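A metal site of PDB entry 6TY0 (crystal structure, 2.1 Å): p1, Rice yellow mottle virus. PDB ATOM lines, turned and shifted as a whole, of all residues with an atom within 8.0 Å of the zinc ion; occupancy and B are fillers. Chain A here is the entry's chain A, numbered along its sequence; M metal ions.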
ATOM      1  N   THR A  35       1.390   1.573 -28.430  1.00  0.00           N
ATOM      2  CA  THR A  35       2.636   0.840 -28.557  1.00  0.00           C
ATOM      3  C   THR A  35       2.419  -0.685 -28.510  1.00  0.00           C
ATOM      4  O   THR A  35       3.081  -1.422 -29.239  1.00  0.00           O
ATOM      5  CB  THR A  35       3.654   1.357 -27.545  1.00  0.00           C
ATOM      6  OG1 THR A  35       3.830   2.739 -27.781  1.00  0.00           O
ATOM      7  CG2 THR A  35       5.017   0.654 -27.627  1.00  0.00           C
ATOM      8  N   TRP A  36       1.434  -1.137 -27.735  1.00  0.00           N
ATOM      9  CA  TRP A  36       1.273  -2.567 -27.448  1.00  0.00           C
ATOM     10  C   TRP A  36       0.028  -3.180 -28.084  1.00  0.00           C
ATOM     11  O   TRP A  36      -0.360  -4.307 -27.749  1.00  0.00           O
ATOM     12  CB  TRP A  36       1.272  -2.775 -25.936  1.00  0.00           C
ATOM     13  CG  TRP A  36       2.422  -2.097 -25.304  1.00  0.00           C
ATOM     14  CD1 TRP A  36       2.384  -0.943 -24.601  1.00  0.00           C
ATOM     15  CD2 TRP A  36       3.784  -2.462 -25.418  1.00  0.00           C
ATOM     16  NE1 TRP A  36       3.632  -0.607 -24.218  1.00  0.00           N
ATOM     17  CE2 TRP A  36       4.526  -1.517 -24.715  1.00  0.00           C
ATOM     18  CE3 TRP A  36       4.468  -3.529 -26.036  1.00  0.00           C
ATOM     19  CZ2 TRP A  36       5.900  -1.572 -24.595  1.00  0.00           C
ATOM     20  CZ3 TRP A  36       5.835  -3.585 -25.904  1.00  0.00           C
ATOM     21  CH2 TRP A  36       6.536  -2.620 -25.197  1.00  0.00           C
ATOM     22  N   ALA A  63       7.426  -5.551 -22.748  1.00  0.00           N
ATOM     23  CA  ALA A  63       8.770  -5.127 -23.208  1.00  0.00           C
ATOM     24  C   ALA A  63       8.965  -5.520 -24.667  1.00  0.00           C
ATOM     25  O   ALA A  63       8.636  -6.662 -25.012  1.00  0.00           O
ATOM     26  CB  ALA A  63       9.812  -5.802 -22.355  1.00  0.00           C
ATOM     27  N   CYS A  64       9.518  -4.632 -25.494  1.00  0.00           N
ATOM     28  CA  CYS A  64       9.827  -4.974 -26.915  1.00  0.00           C
ATOM     29  C   CYS A  64      11.109  -5.786 -26.991  1.00  0.00           C
ATOM     30  O   CYS A  64      12.114  -5.421 -26.398  1.00  0.00           O
ATOM     31  CB  CYS A  64       9.994  -3.723 -27.778  1.00  0.00           C
ATOM     32  SG  CYS A  64      10.194  -4.015 -29.591  1.00  0.00           S
ATOM     33  N   THR A  65      11.106  -6.848 -27.762  1.00  0.00           N
ATOM     34  CA  THR A  65      12.327  -7.622 -28.015  1.00  0.00           C
ATOM     35  C   THR A  65      13.330  -6.952 -28.981  1.00  0.00           C
ATOM     36  O   THR A  65      14.469  -7.402 -29.077  1.00  0.00           O
ATOM     37  CB  THR A  65      11.944  -8.986 -28.558  1.00  0.00           C
ATOM     38  OG1 THR A  65      11.146  -8.790 -29.731  1.00  0.00           O
ATOM     39  CG2 THR A  65      11.115  -9.753 -27.529  1.00  0.00           C
ATOM     40  N   GLN A  66      12.955  -5.845 -29.630  1.00  0.00           N
ATOM     41  CA  GLN A  66      13.792  -5.173 -30.633  1.00  0.00           C
ATOM     42  C   GLN A  66      14.289  -3.832 -30.168  1.00  0.00           C
ATOM     43  O   GLN A  66      15.375  -3.412 -30.545  1.00  0.00           O
ATOM     44  CB  GLN A  66      13.013  -4.890 -31.925  1.00  0.00           C
ATOM     45  CG  GLN A  66      12.397  -6.097 -32.588  1.00  0.00           C
ATOM     46  CD  GLN A  66      13.455  -7.094 -32.871  1.00  0.00           C
ATOM     47  OE1 GLN A  66      14.287  -6.884 -33.755  1.00  0.00           O
ATOM     48  NE2 GLN A  66      13.493  -8.158 -32.090  1.00  0.00           N
ATOM     49  N   CYS A  67      13.489  -3.079 -29.449  1.00  0.00           N
ATOM     50  CA  CYS A  67      13.966  -1.813 -28.948  1.00  0.00           C
ATOM     51  C   CYS A  67      13.822  -1.972 -27.462  1.00  0.00           C
ATOM     52  O   CYS A  67      13.624  -3.087 -26.968  1.00  0.00           O
ATOM     53  CB  CYS A  67      13.185  -0.641 -29.525  1.00  0.00           C
ATOM     54  SG  CYS A  67      11.428  -0.467 -29.046  1.00  0.00           S
ATOM     55  N   THR A  68      13.941  -0.899 -26.721  1.00  0.00           N
ATOM     56  CA  THR A  68      13.824  -1.091 -25.290  1.00  0.00           C
ATOM     57  C   THR A  68      12.523  -0.494 -24.769  1.00  0.00           C
ATOM     58  O   THR A  68      12.402  -0.198 -23.566  1.00  0.00           O
ATOM     59  CB  THR A  68      14.990  -0.422 -24.601  1.00  0.00           C
ATOM     60  OG1 THR A  68      15.005   0.924 -25.039  1.00  0.00           O
ATOM     61  CG2 THR A  68      16.276  -1.088 -24.991  1.00  0.00           C
ATOM     62  N   ALA A  69      11.560  -0.314 -25.646  1.00  0.00           N
ATOM     63  CA  ALA A  69      10.239   0.122 -25.198  1.00  0.00           C
ATOM     64  C   ALA A  69       9.738  -0.855 -24.115  1.00  0.00           C
ATOM     65  O   ALA A  69       9.884  -2.064 -24.247  1.00  0.00           O
ATOM     66  CB  ALA A  69       9.312   0.119 -26.355  1.00  0.00           C
ATOM     67  N   HIS A  70       9.161  -0.321 -23.051  1.00  0.00           N
ATOM     68  CA  HIS A  70       8.651  -1.153 -21.996  1.00  0.00           C
ATOM     69  C   HIS A  70       7.566  -0.428 -21.222  1.00  0.00           C
ATOM     70  O   HIS A  70       7.470   0.797 -21.280  1.00  0.00           O
ATOM     71  CB  HIS A  70       9.806  -1.568 -21.072  1.00  0.00           C
ATOM     72  CG  HIS A  70      10.416  -0.429 -20.355  1.00  0.00           C
ATOM     73  ND1 HIS A  70      11.351   0.409 -20.930  1.00  0.00           N
ATOM     74  CD2 HIS A  70      10.229   0.031 -19.086  1.00  0.00           C
ATOM     75  CE1 HIS A  70      11.708   1.331 -20.048  1.00  0.00           C
ATOM     76  NE2 HIS A  70      11.025   1.134 -18.931  1.00  0.00           N
ATOM     77  N   VAL A  90       7.352  -8.921 -26.637  1.00  0.00           N
ATOM     78  CA  VAL A  90       6.803  -8.933 -27.965  1.00  0.00           C
ATOM     79  C   VAL A  90       7.533  -7.925 -28.824  1.00  0.00           C
ATOM     80  O   VAL A  90       8.392  -7.226 -28.338  1.00  0.00           O
ATOM     81  CB  VAL A  90       5.308  -8.564 -27.918  1.00  0.00           C
ATOM     82  CG1 VAL A  90       4.544  -9.569 -27.070  1.00  0.00           C
ATOM     83  CG2 VAL A  90       5.102  -7.145 -27.401  1.00  0.00           C
ATOM     84  N   VAL A  91       7.205  -7.881 -30.101  1.00  0.00           N
ATOM     85  CA  VAL A  91       7.714  -6.848 -31.009  1.00  0.00           C
ATOM     86  C   VAL A  91       6.668  -5.745 -30.976  1.00  0.00           C
ATOM     87  O   VAL A  91       5.496  -5.995 -31.273  1.00  0.00           O
ATOM     88  CB  VAL A  91       7.937  -7.387 -32.446  1.00  0.00           C
ATOM     89  CG1 VAL A  91       8.411  -6.281 -33.365  1.00  0.00           C
ATOM     90  CG2 VAL A  91       8.924  -8.556 -32.431  1.00  0.00           C
ATOM     91  N   CYS A  92       7.106  -4.549 -30.611  1.00  0.00           N
ATOM     92  CA  CYS A  92       6.157  -3.437 -30.383  1.00  0.00           C
ATOM     93  C   CYS A  92       5.651  -2.892 -31.732  1.00  0.00           C
ATOM     94  O   CYS A  92       6.142  -3.300 -32.804  1.00  0.00           O
ATOM     95  CB  CYS A  92       6.818  -2.325 -29.558  1.00  0.00           C
ATOM     96  SG  CYS A  92       7.870  -1.197 -30.562  1.00  0.00           S
ATOM     97  N   ALA A  93       4.640  -2.023 -31.692  1.00  0.00           N
ATOM     98  CA  ALA A  93       4.033  -1.482 -32.919  1.00  0.00           C
ATOM     99  C   ALA A  93       5.018  -0.692 -33.799  1.00  0.00           C
ATOM    100  O   ALA A  93       4.852  -0.617 -34.980  1.00  0.00           O
ATOM    101  CB  ALA A  93       2.799  -0.636 -32.599  1.00  0.00           C
ATOM    102  N   ASP A  94       6.035  -0.081 -33.235  1.00  0.00           N
ATOM    103  CA  ASP A  94       6.958   0.655 -34.074  1.00  0.00           C
ATOM    104  C   ASP A  94       7.923  -0.290 -34.764  1.00  0.00           C
ATOM    105  O   ASP A  94       8.342  -0.051 -35.895  1.00  0.00           O
ATOM    106  CB  ASP A  94       7.697   1.696 -33.271  1.00  0.00           C
ATOM    107  CG  ASP A  94       6.742   2.632 -32.586  1.00  0.00           C
ATOM    108  OD1 ASP A  94       5.928   3.247 -33.292  1.00  0.00           O
ATOM    109  OD2 ASP A  94       6.758   2.705 -31.340  1.00  0.00           O
ATOM    110  N   CYS A  95       8.253  -1.370 -34.088  1.00  0.00           N
ATOM    111  CA  CYS A  95       9.257  -2.286 -34.564  1.00  0.00           C
ATOM    112  C   CYS A  95       8.700  -3.295 -35.570  1.00  0.00           C
ATOM    113  O   CYS A  95       9.454  -3.792 -36.373  1.00  0.00           O
ATOM    114  CB  CYS A  95       9.958  -2.967 -33.375  1.00  0.00           C
ATOM    115  SG  CYS A  95      11.063  -1.824 -32.522  1.00  0.00           S
ATOM    116  N   GLU A  96       7.406  -3.600 -35.526  1.00  0.00           N
ATOM    117  CA  GLU A  96       6.721  -4.365 -36.575  1.00  0.00           C
ATOM    118  C   GLU A  96       6.975  -3.881 -38.032  1.00  0.00           C
ATOM    119  O   GLU A  96       7.068  -4.684 -38.937  1.00  0.00           O
ATOM    120  CB  GLU A  96       5.216  -4.229 -36.383  1.00  0.00           C
ATOM    121  CG  GLU A  96       4.586  -5.183 -35.428  1.00  0.00           C
ATOM    122  CD  GLU A  96       3.092  -4.962 -35.342  1.00  0.00           C
ATOM    123  OE1 GLU A  96       2.623  -3.833 -35.624  1.00  0.00           O
ATOM    124  OE2 GLU A  96       2.372  -5.916 -35.003  1.00  0.00           O
HETATM  125 ZN    ZN M   1      10.153  -1.877 -30.322  1.00  0.00          ZN
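The zinc ion is bound by SG of Cys 64 (2.3 Å). The zinc ion is bound by SG of Cys 67 (2.3 Å). The zinc ion is bound by the side-chain sulfur (SG) of Cys 95, at 2.4 Å. The zinc ion is bound by the side-chain sulfur (SG) of Cys 92.
The side-chain sulfur (SG) of Cys 67 sits close to the backbone NH (N) of Ala 69, 3.4 Å away. The side-chain sulfur (SG) of Cys 64 sits close to the backbone NH (N) of Gln 66. The backbone NH (N) of Cys 64 sits at hydrogen-bond distance from the backbone carbonyl oxygen (O) of Ala 69, 2.9 Å away. The backbone NH (N) of Asp 94 sits close to the side-chain sulfur (SG) of Cys 92 (3.4 Å).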
